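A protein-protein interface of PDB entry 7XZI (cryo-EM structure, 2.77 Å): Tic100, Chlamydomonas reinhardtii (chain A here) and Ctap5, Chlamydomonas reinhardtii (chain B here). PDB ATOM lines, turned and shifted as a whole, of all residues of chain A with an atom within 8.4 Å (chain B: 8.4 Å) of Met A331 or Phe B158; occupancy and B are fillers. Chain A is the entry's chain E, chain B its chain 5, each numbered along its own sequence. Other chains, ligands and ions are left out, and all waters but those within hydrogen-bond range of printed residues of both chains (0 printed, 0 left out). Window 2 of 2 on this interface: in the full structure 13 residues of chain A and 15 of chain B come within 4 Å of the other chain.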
ATOM      1  N   PRO A 299      14.391  -8.050  -4.052  1.00  0.00           N
ATOM      2  CA  PRO A 299      13.458  -7.592  -5.097  1.00  0.00           C
ATOM      3  C   PRO A 299      14.068  -7.532  -6.485  1.00  0.00           C
ATOM      4  O   PRO A 299      13.333  -7.682  -7.469  1.00  0.00           O
ATOM      5  CB  PRO A 299      13.047  -6.196  -4.613  1.00  0.00           C
ATOM      6  CG  PRO A 299      13.229  -6.247  -3.143  1.00  0.00           C
ATOM      7  CD  PRO A 299      14.421  -7.126  -2.905  1.00  0.00           C
ATOM      8  N   ASP A 300      15.377  -7.319  -6.599  1.00  0.00           N
ATOM      9  CA  ASP A 300      16.052  -7.363  -7.890  1.00  0.00           C
ATOM     10  C   ASP A 300      16.431  -8.777  -8.306  1.00  0.00           C
ATOM     11  O   ASP A 300      17.202  -8.939  -9.257  1.00  0.00           O
ATOM     12  CB  ASP A 300      17.300  -6.474  -7.859  1.00  0.00           C
ATOM     13  CG  ASP A 300      18.293  -6.897  -6.797  1.00  0.00           C
ATOM     14  OD1 ASP A 300      17.887  -7.599  -5.851  1.00  0.00           O
ATOM     15  OD2 ASP A 300      19.479  -6.521  -6.901  1.00  0.00           O
ATOM     16  N   PHE A 301      15.924  -9.790  -7.603  1.00  0.00           N
ATOM     17  CA  PHE A 301      16.124 -11.219  -7.852  1.00  0.00           C
ATOM     18  C   PHE A 301      17.548 -11.668  -7.563  1.00  0.00           C
ATOM     19  O   PHE A 301      17.923 -12.784  -7.948  1.00  0.00           O
ATOM     20  CB  PHE A 301      15.739 -11.632  -9.277  1.00  0.00           C
ATOM     21  CG  PHE A 301      14.268 -11.875  -9.455  1.00  0.00           C
ATOM     22  CD1 PHE A 301      13.393 -11.681  -8.400  1.00  0.00           C
ATOM     23  CD2 PHE A 301      13.762 -12.312 -10.667  1.00  0.00           C
ATOM     24  CE1 PHE A 301      12.042 -11.905  -8.552  1.00  0.00           C
ATOM     25  CE2 PHE A 301      12.408 -12.539 -10.824  1.00  0.00           C
ATOM     26  CZ  PHE A 301      11.548 -12.335  -9.766  1.00  0.00           C
ATOM     27  N   THR A 302      18.356 -10.844  -6.904  1.00  0.00           N
ATOM     28  CA  THR A 302      19.620 -11.325  -6.370  1.00  0.00           C
ATOM     29  C   THR A 302      19.339 -12.259  -5.202  1.00  0.00           C
ATOM     30  O   THR A 302      18.562 -11.925  -4.303  1.00  0.00           O
ATOM     31  CB  THR A 302      20.493 -10.154  -5.925  1.00  0.00           C
ATOM     32  OG1 THR A 302      20.811  -9.339  -7.060  1.00  0.00           O
ATOM     33  CG2 THR A 302      21.781 -10.653  -5.289  1.00  0.00           C
ATOM     34  N   GLY A 322      21.294 -11.060  -9.889  1.00  0.00           N
ATOM     35  CA  GLY A 322      20.319 -10.745 -10.911  1.00  0.00           C
ATOM     36  C   GLY A 322      20.580  -9.353 -11.443  1.00  0.00           C
ATOM     37  O   GLY A 322      21.739  -8.958 -11.597  1.00  0.00           O
ATOM     38  N   THR A 323      19.523  -8.601 -11.736  1.00  0.00           N
ATOM     39  CA  THR A 323      19.698  -7.187 -12.037  1.00  0.00           C
ATOM     40  C   THR A 323      20.242  -6.472 -10.808  1.00  0.00           C
ATOM     41  O   THR A 323      19.836  -6.752  -9.677  1.00  0.00           O
ATOM     42  CB  THR A 323      18.373  -6.564 -12.471  1.00  0.00           C
ATOM     43  OG1 THR A 323      17.414  -6.699 -11.416  1.00  0.00           O
ATOM     44  CG2 THR A 323      17.844  -7.253 -13.719  1.00  0.00           C
ATOM     45  N   GLY A 324      21.168  -5.552 -11.027  1.00  0.00           N
ATOM     46  CA  GLY A 324      21.865  -4.907  -9.936  1.00  0.00           C
ATOM     47  C   GLY A 324      23.160  -5.609  -9.580  1.00  0.00           C
ATOM     48  O   GLY A 324      23.829  -6.218 -10.418  1.00  0.00           O
ATOM     49  N   THR A 325      23.513  -5.517  -8.301  1.00  0.00           N
ATOM     50  CA  THR A 325      24.742  -6.120  -7.798  1.00  0.00           C
ATOM     51  C   THR A 325      24.552  -6.463  -6.324  1.00  0.00           C
ATOM     52  O   THR A 325      23.456  -6.327  -5.772  1.00  0.00           O
ATOM     53  CB  THR A 325      25.936  -5.184  -8.013  1.00  0.00           C
ATOM     54  OG1 THR A 325      27.142  -5.846  -7.610  1.00  0.00           O
ATOM     55  CG2 THR A 325      25.770  -3.914  -7.195  1.00  0.00           C
ATOM     56  N   GLY A 326      25.627  -6.910  -5.689  1.00  0.00           N
ATOM     57  CA  GLY A 326      25.594  -7.242  -4.277  1.00  0.00           C
ATOM     58  C   GLY A 326      26.952  -7.735  -3.828  1.00  0.00           C
ATOM     59  O   GLY A 326      27.882  -7.880  -4.628  1.00  0.00           O
ATOM     60  N   GLY A 328      29.224  -6.280  -2.291  1.00  0.00           N
ATOM     61  CA  GLY A 328      30.294  -5.320  -2.452  1.00  0.00           C
ATOM     62  C   GLY A 328      30.845  -5.193  -3.855  1.00  0.00           C
ATOM     63  O   GLY A 328      31.723  -4.351  -4.082  1.00  0.00           O
ATOM     64  N   PHE A 329      30.366  -5.996  -4.799  1.00  0.00           N
ATOM     65  CA  PHE A 329      30.850  -5.910  -6.168  1.00  0.00           C
ATOM     66  C   PHE A 329      30.397  -4.608  -6.816  1.00  0.00           C
ATOM     67  O   PHE A 329      29.377  -4.023  -6.444  1.00  0.00           O
ATOM     68  CB  PHE A 329      30.357  -7.100  -6.991  1.00  0.00           C
ATOM     69  CG  PHE A 329      31.076  -8.389  -6.697  1.00  0.00           C
ATOM     70  CD1 PHE A 329      32.086  -8.438  -5.752  1.00  0.00           C
ATOM     71  CD2 PHE A 329      30.748  -9.547  -7.379  1.00  0.00           C
ATOM     72  CE1 PHE A 329      32.746  -9.621  -5.485  1.00  0.00           C
ATOM     73  CE2 PHE A 329      31.406 -10.733  -7.117  1.00  0.00           C
ATOM     74  CZ  PHE A 329      32.407 -10.769  -6.169  1.00  0.00           C
ATOM     75  N   ALA A 330      31.178  -4.150  -7.791  1.00  0.00           N
ATOM     76  CA  ALA A 330      30.797  -2.973  -8.556  1.00  0.00           C
ATOM     77  C   ALA A 330      29.582  -3.278  -9.424  1.00  0.00           C
ATOM     78  O   ALA A 330      29.311  -4.429  -9.773  1.00  0.00           O
ATOM     79  CB  ALA A 330      31.959  -2.496  -9.425  1.00  0.00           C
ATOM     80  N   MET A 331      28.843  -2.221  -9.767  1.00  0.00           N
ATOM     81  CA  MET A 331      27.605  -2.387 -10.522  1.00  0.00           C
ATOM     82  C   MET A 331      27.858  -2.931 -11.922  1.00  0.00           C
ATOM     83  O   MET A 331      26.990  -3.605 -12.489  1.00  0.00           O
ATOM     84  CB  MET A 331      26.865  -1.052 -10.599  1.00  0.00           C
ATOM     85  CG  MET A 331      25.410  -1.151 -11.025  1.00  0.00           C
ATOM     86  SD  MET A 331      24.346  -1.762  -9.704  1.00  0.00           S
ATOM     87  CE  MET A 331      22.728  -1.401 -10.377  1.00  0.00           C
ATOM     88  N   SER A 332      29.027  -2.651 -12.496  1.00  0.00           N
ATOM     89  CA  SER A 332      29.334  -3.056 -13.861  1.00  0.00           C
ATOM     90  C   SER A 332      30.013  -4.417 -13.953  1.00  0.00           C
ATOM     91  O   SER A 332      30.171  -4.935 -15.063  1.00  0.00           O
ATOM     92  CB  SER A 332      30.225  -2.007 -14.532  1.00  0.00           C
ATOM     93  OG  SER A 332      31.442  -1.850 -13.826  1.00  0.00           O
ATOM     94  N   GLN A 333      30.417  -5.006 -12.826  1.00  0.00           N
ATOM     95  CA  GLN A 333      31.139  -6.273 -12.878  1.00  0.00           C
ATOM     96  C   GLN A 333      30.208  -7.441 -13.177  1.00  0.00           C
ATOM     97  O   GLN A 333      30.574  -8.358 -13.922  1.00  0.00           O
ATOM     98  CB  GLN A 333      31.882  -6.508 -11.564  1.00  0.00           C
ATOM     99  CG  GLN A 333      32.970  -5.492 -11.279  1.00  0.00           C
ATOM    100  CD  GLN A 333      33.742  -5.806 -10.014  1.00  0.00           C
ATOM    101  OE1 GLN A 333      33.737  -6.941  -9.535  1.00  0.00           O
ATOM    102  NE2 GLN A 333      34.407  -4.799  -9.462  1.00  0.00           N
ATOM    103  N   THR A 334      29.009  -7.430 -12.611  1.00  0.00           N
ATOM    104  CA  THR A 334      28.124  -8.584 -12.640  1.00  0.00           C
ATOM    105  C   THR A 334      27.103  -8.481 -13.767  1.00  0.00           C
ATOM    106  O   THR A 334      26.846  -7.407 -14.318  1.00  0.00           O
ATOM    107  CB  THR A 334      27.399  -8.736 -11.302  1.00  0.00           C
ATOM    108  OG1 THR A 334      26.519  -7.624 -11.109  1.00  0.00           O
ATOM    109  CG2 THR A 334      28.403  -8.778 -10.162  1.00  0.00           C
ATOM    110  N   ARG A 335      26.523  -9.629 -14.104  1.00  0.00           N
ATOM    111  CA  ARG A 335      25.424  -9.740 -15.049  1.00  0.00           C
ATOM    112  C   ARG A 335      24.352 -10.632 -14.434  1.00  0.00           C
ATOM    113  O   ARG A 335      24.486 -11.107 -13.303  1.00  0.00           O
ATOM    114  CB  ARG A 335      25.896 -10.295 -16.399  1.00  0.00           C
ATOM    115  CG  ARG A 335      26.798  -9.355 -17.180  1.00  0.00           C
ATOM    116  CD  ARG A 335      26.066  -8.077 -17.557  1.00  0.00           C
ATOM    117  NE  ARG A 335      26.911  -7.166 -18.314  1.00  0.00           N
ATOM    118  CZ  ARG A 335      27.703  -6.247 -17.769  1.00  0.00           C
ATOM    119  NH1 ARG A 335      27.783  -6.096 -16.458  1.00  0.00           N
ATOM    120  NH2 ARG A 335      28.429  -5.465 -18.561  1.00  0.00           N
ATOM    121  N   ALA B 155      16.432   9.466  -9.327  1.00  0.00           N
ATOM    122  CA  ALA B 155      15.844   8.322 -10.021  1.00  0.00           C
ATOM    123  C   ALA B 155      16.881   7.739 -10.966  1.00  0.00           C
ATOM    124  O   ALA B 155      17.399   8.454 -11.830  1.00  0.00           O
ATOM    125  CB  ALA B 155      14.589   8.734 -10.787  1.00  0.00           C
ATOM    126  N   TYR B 156      17.182   6.453 -10.808  1.00  0.00           N
ATOM    127  CA  TYR B 156      18.095   5.743 -11.690  1.00  0.00           C
ATOM    128  C   TYR B 156      17.449   4.438 -12.136  1.00  0.00           C
ATOM    129  O   TYR B 156      16.487   3.956 -11.531  1.00  0.00           O
ATOM    130  CB  TYR B 156      19.449   5.480 -11.013  1.00  0.00           C
ATOM    131  CG  TYR B 156      19.357   4.841  -9.646  1.00  0.00           C
ATOM    132  CD1 TYR B 156      19.134   5.610  -8.512  1.00  0.00           C
ATOM    133  CD2 TYR B 156      19.511   3.472  -9.488  1.00  0.00           C
ATOM    134  CE1 TYR B 156      19.055   5.029  -7.260  1.00  0.00           C
ATOM    135  CE2 TYR B 156      19.436   2.887  -8.241  1.00  0.00           C
ATOM    136  CZ  TYR B 156      19.207   3.667  -7.132  1.00  0.00           C
ATOM    137  OH  TYR B 156      19.132   3.080  -5.890  1.00  0.00           O
ATOM    138  N   SER B 157      17.991   3.861 -13.210  1.00  0.00           N
ATOM    139  CA  SER B 157      17.364   2.729 -13.882  1.00  0.00           C
ATOM    140  C   SER B 157      18.257   1.494 -13.925  1.00  0.00           C
ATOM    141  O   SER B 157      18.080   0.643 -14.802  1.00  0.00           O
ATOM    142  CB  SER B 157      16.952   3.124 -15.302  1.00  0.00           C
ATOM    143  OG  SER B 157      18.075   3.567 -16.043  1.00  0.00           O
ATOM    144  N   PHE B 158      19.232   1.389 -13.022  1.00  0.00           N
ATOM    145  CA  PHE B 158      20.109   0.226 -12.880  1.00  0.00           C
ATOM    146  C   PHE B 158      20.971  -0.026 -14.111  1.00  0.00           C
ATOM    147  O   PHE B 158      21.721  -1.008 -14.138  1.00  0.00           O
ATOM    148  CB  PHE B 158      19.329  -1.053 -12.557  1.00  0.00           C
ATOM    149  CG  PHE B 158      18.832  -1.130 -11.142  1.00  0.00           C
ATOM    150  CD1 PHE B 158      19.267  -0.231 -10.184  1.00  0.00           C
ATOM    151  CD2 PHE B 158      17.935  -2.116 -10.770  1.00  0.00           C
ATOM    152  CE1 PHE B 158      18.806  -0.314  -8.884  1.00  0.00           C
ATOM    153  CE2 PHE B 158      17.473  -2.201  -9.474  1.00  0.00           C
ATOM    154  CZ  PHE B 158      17.909  -1.299  -8.529  1.00  0.00           C
ATOM    155  N   ALA B 159      20.880   0.816 -15.133  1.00  0.00           N
ATOM    156  CA  ALA B 159      21.668   0.664 -16.348  1.00  0.00           C
ATOM    157  C   ALA B 159      22.683   1.776 -16.532  1.00  0.00           C
ATOM    158  O   ALA B 159      23.761   1.537 -17.084  1.00  0.00           O
ATOM    159  CB  ALA B 159      20.749   0.601 -17.575  1.00  0.00           C
ATOM    160  N   GLN B 160      22.364   2.992 -16.086  1.00  0.00           N
ATOM    161  CA  GLN B 160      23.346   4.067 -16.088  1.00  0.00           C
ATOM    162  C   GLN B 160      24.493   3.787 -15.128  1.00  0.00           C
ATOM    163  O   GLN B 160      25.592   4.323 -15.314  1.00  0.00           O
ATOM    164  CB  GLN B 160      22.669   5.394 -15.736  1.00  0.00           C
ATOM    165  CG  GLN B 160      21.975   5.403 -14.383  1.00  0.00           C
ATOM    166  CD  GLN B 160      21.195   6.680 -14.134  1.00  0.00           C
ATOM    167  OE1 GLN B 160      20.370   7.087 -14.952  1.00  0.00           O
ATOM    168  NE2 GLN B 160      21.456   7.321 -13.002  1.00  0.00           N
ATOM    169  N   LEU B 161      24.263   2.959 -14.110  1.00  0.00           N
ATOM    170  CA  LEU B 161      25.312   2.550 -13.188  1.00  0.00           C
ATOM    171  C   LEU B 161      26.038   1.287 -13.634  1.00  0.00           C
ATOM    172  O   LEU B 161      27.097   0.974 -13.081  1.00  0.00           O
ATOM    173  CB  LEU B 161      24.727   2.327 -11.789  1.00  0.00           C
ATOM    174  CG  LEU B 161      24.067   3.529 -11.110  1.00  0.00           C
ATOM    175  CD1 LEU B 161      23.391   3.107  -9.817  1.00  0.00           C
ATOM    176  CD2 LEU B 161      25.092   4.618 -10.847  1.00  0.00           C
ATOM    177  N   LYS B 162      25.506   0.565 -14.619  1.00  0.00           N
ATOM    178  CA  LYS B 162      26.095  -0.685 -15.082  1.00  0.00           C
ATOM    179  C   LYS B 162      26.822  -0.541 -16.409  1.00  0.00           C
ATOM    180  O   LYS B 162      27.986  -0.935 -16.522  1.00  0.00           O
ATOM    181  CB  LYS B 162      25.009  -1.765 -15.197  1.00  0.00           C
ATOM    182  CG  LYS B 162      25.535  -3.126 -15.618  1.00  0.00           C
ATOM    183  CD  LYS B 162      24.429  -4.168 -15.629  1.00  0.00           C
ATOM    184  CE  LYS B 162      23.836  -4.358 -14.245  1.00  0.00           C
ATOM    185  NZ  LYS B 162      24.860  -4.798 -13.259  1.00  0.00           N
ATOM    186  N   TYR B 163      26.168   0.015 -17.424  1.00  0.00           N
ATOM    187  CA  TYR B 163      26.788   0.206 -18.728  1.00  0.00           C
ATOM    188  C   TYR B 163      27.315   1.632 -18.839  1.00  0.00           C
ATOM    189  O   TYR B 163      26.553   2.594 -18.703  1.00  0.00           O
ATOM    190  CB  TYR B 163      25.791  -0.087 -19.848  1.00  0.00           C
ATOM    191  CG  TYR B 163      25.168  -1.462 -19.755  1.00  0.00           C
ATOM    192  CD1 TYR B 163      25.797  -2.568 -20.309  1.00  0.00           C
ATOM    193  CD2 TYR B 163      23.954  -1.653 -19.111  1.00  0.00           C
ATOM    194  CE1 TYR B 163      25.233  -3.825 -20.226  1.00  0.00           C
ATOM    195  CE2 TYR B 163      23.383  -2.908 -19.022  1.00  0.00           C
ATOM    196  CZ  TYR B 163      24.027  -3.989 -19.581  1.00  0.00           C
ATOM    197  OH  TYR B 163      23.463  -5.241 -19.497  1.00  0.00           O
ATOM    198  N   LYS B 164      28.615   1.760 -19.091  1.00  0.00           N
ATOM    199  CA  LYS B 164      29.289   3.051 -19.104  1.00  0.00           C
ATOM    200  C   LYS B 164      29.377   3.672 -20.492  1.00  0.00           C
ATOM    201  O   LYS B 164      29.902   4.783 -20.623  1.00  0.00           O
ATOM    202  CB  LYS B 164      30.697   2.911 -18.514  1.00  0.00           C
ATOM    203  CG  LYS B 164      30.729   2.325 -17.111  1.00  0.00           C
ATOM    204  CD  LYS B 164      32.154   2.170 -16.606  1.00  0.00           C
ATOM    205  N   LEU B 166      26.606   4.134 -22.535  1.00  0.00           N
ATOM    206  CA  LEU B 166      25.270   4.520 -22.965  1.00  0.00           C
ATOM    207  C   LEU B 166      25.260   5.964 -23.449  1.00  0.00           C
ATOM    208  O   LEU B 166      25.849   6.847 -22.817  1.00  0.00           O
ATOM    209  CB  LEU B 166      24.273   4.342 -21.821  1.00  0.00           C
ATOM    210  CG  LEU B 166      23.941   2.913 -21.391  1.00  0.00           C
ATOM    211  CD1 LEU B 166      22.985   2.922 -20.209  1.00  0.00           C
ATOM    212  CD2 LEU B 166      23.349   2.137 -22.552  1.00  0.00           C
ATOM    213  N   PHE B 174      16.085   4.501 -20.980  1.00  0.00           N
ATOM    214  CA  PHE B 174      16.080   3.620 -19.815  1.00  0.00           C
ATOM    215  C   PHE B 174      15.500   4.320 -18.592  1.00  0.00           C
ATOM    216  O   PHE B 174      14.736   3.718 -17.824  1.00  0.00           O
ATOM    217  CB  PHE B 174      17.495   3.119 -19.526  1.00  0.00           C
ATOM    218  CG  PHE B 174      17.847   1.849 -20.244  1.00  0.00           C
ATOM    219  CD1 PHE B 174      17.534   0.620 -19.691  1.00  0.00           C
ATOM    220  CD2 PHE B 174      18.492   1.882 -21.467  1.00  0.00           C
ATOM    221  CE1 PHE B 174      17.853  -0.552 -20.343  1.00  0.00           C
ATOM    222  CE2 PHE B 174      18.815   0.711 -22.125  1.00  0.00           C
ATOM    223  CZ  PHE B 174      18.496  -0.506 -21.562  1.00  0.00           C
ATOM    224  N   HIS B 175      15.849   5.595 -18.398  1.00  0.00           N
ATOM    225  CA  HIS B 175      15.369   6.341 -17.242  1.00  0.00           C
ATOM    226  C   HIS B 175      13.854   6.471 -17.261  1.00  0.00           C
ATOM    227  O   HIS B 175      13.206   6.350 -16.218  1.00  0.00           O
ATOM    228  CB  HIS B 175      16.025   7.722 -17.203  1.00  0.00           C
ATOM    229  CG  HIS B 175      15.499   8.615 -16.123  1.00  0.00           C
ATOM    230  ND1 HIS B 175      15.971   8.577 -14.829  1.00  0.00           N
ATOM    231  CD2 HIS B 175      14.544   9.574 -16.147  1.00  0.00           C
ATOM    232  CE1 HIS B 175      15.329   9.473 -14.101  1.00  0.00           C
ATOM    233  NE2 HIS B 175      14.457  10.091 -14.877  1.00  0.00           N
ATOM    234  N   TYR B 178      12.245   2.454 -16.889  1.00  0.00           N
ATOM    235  CA  TYR B 178      12.304   1.719 -15.633  1.00  0.00           C
ATOM    236  C   TYR B 178      12.307   2.601 -14.393  1.00  0.00           C
ATOM    237  O   TYR B 178      12.265   2.069 -13.280  1.00  0.00           O
ATOM    238  CB  TYR B 178      13.534   0.803 -15.615  1.00  0.00           C
ATOM    239  CG  TYR B 178      13.480  -0.264 -16.683  1.00  0.00           C
ATOM    240  CD1 TYR B 178      12.556  -1.297 -16.610  1.00  0.00           C
ATOM    241  CD2 TYR B 178      14.341  -0.234 -17.769  1.00  0.00           C
ATOM    242  CE1 TYR B 178      12.494  -2.270 -17.584  1.00  0.00           C
ATOM    243  CE2 TYR B 178      14.289  -1.205 -18.750  1.00  0.00           C
ATOM    244  CZ  TYR B 178      13.363  -2.221 -18.651  1.00  0.00           C
ATOM    245  OH  TYR B 178      13.302  -3.192 -19.622  1.00  0.00           O
ATOM    246  N   ALA B 179      12.359   3.921 -14.553  1.00  0.00           N
ATOM    247  CA  ALA B 179      12.208   4.861 -13.453  1.00  0.00           C
ATOM    248  C   ALA B 179      11.201   5.931 -13.851  1.00  0.00           C
ATOM    249  O   ALA B 179      10.941   6.153 -15.037  1.00  0.00           O
ATOM    250  CB  ALA B 179      13.547   5.503 -13.067  1.00  0.00           C
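Of chain B, only Phe B158 (3.7 Å), Leu B161 (3.2 Å) and Lys B162 (2.6 Å) come within 4 Å of Met A331. Phe B158 touches just one residue of chain A: Met A331 (3.7 Å). Ala A330 touches none of the printed residues of chain B. No residue of chain A comes within 4 Å of Ser B157. Of the printed residues of chain B, Arg A335 touches Lys B162 (3.8 Å) and Tyr B163 (3.96 Å). Printed residues of chain B within 4 Å of Thr A334: Lys B162 (3.4 Å). Thr A302 touches none of the printed residues of chain B.
O of Gly A324 sits at hydrogen-bond distance from NZ of Lys B162 (3.3 Å). The backbone carbonyl oxygen (O) of Thr A334 lies within hydrogen-bond range of the side-chain amino group (NZ) of Lys B162 (3.4 Å). The side-chain amino group of Lys B162 lies within hydrogen-bond range of the backbone carbonyl oxygen of Met A331, at 2.6 Å.
Printed residues of chain B that touch a printed residue of chain A: Phe B158, Leu B161, Lys B162 and Tyr B163. Of the 17 printed residues of chain A, 5 touch a printed residue of chain B. Among the printed residues, no Asp or Glu carboxylate lies within 4 Å of a Lys or Arg side-chain nitrogen of the other chain.
The backbone carbonyl oxygen of Ser A332 is in hydrogen-bond range of the guanidinium group of Arg A335 (3.0 Å). The side-chain hydroxyl (OG1) of Thr A334 is in hydrogen-bond range of the backbone carbonyl oxygen (O) of Gly A324.
Among the printed residues, pairs that only touch across the chains: Ser A332 with Lys B162 (3.2 Å), Met A331 with Leu B161 (3.2 Å), Met A331 with Phe B158 (3.7 Å), Arg A335 with Lys B162 (3.8 Å) and Arg A335 with Tyr B163 (3.96 Å).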
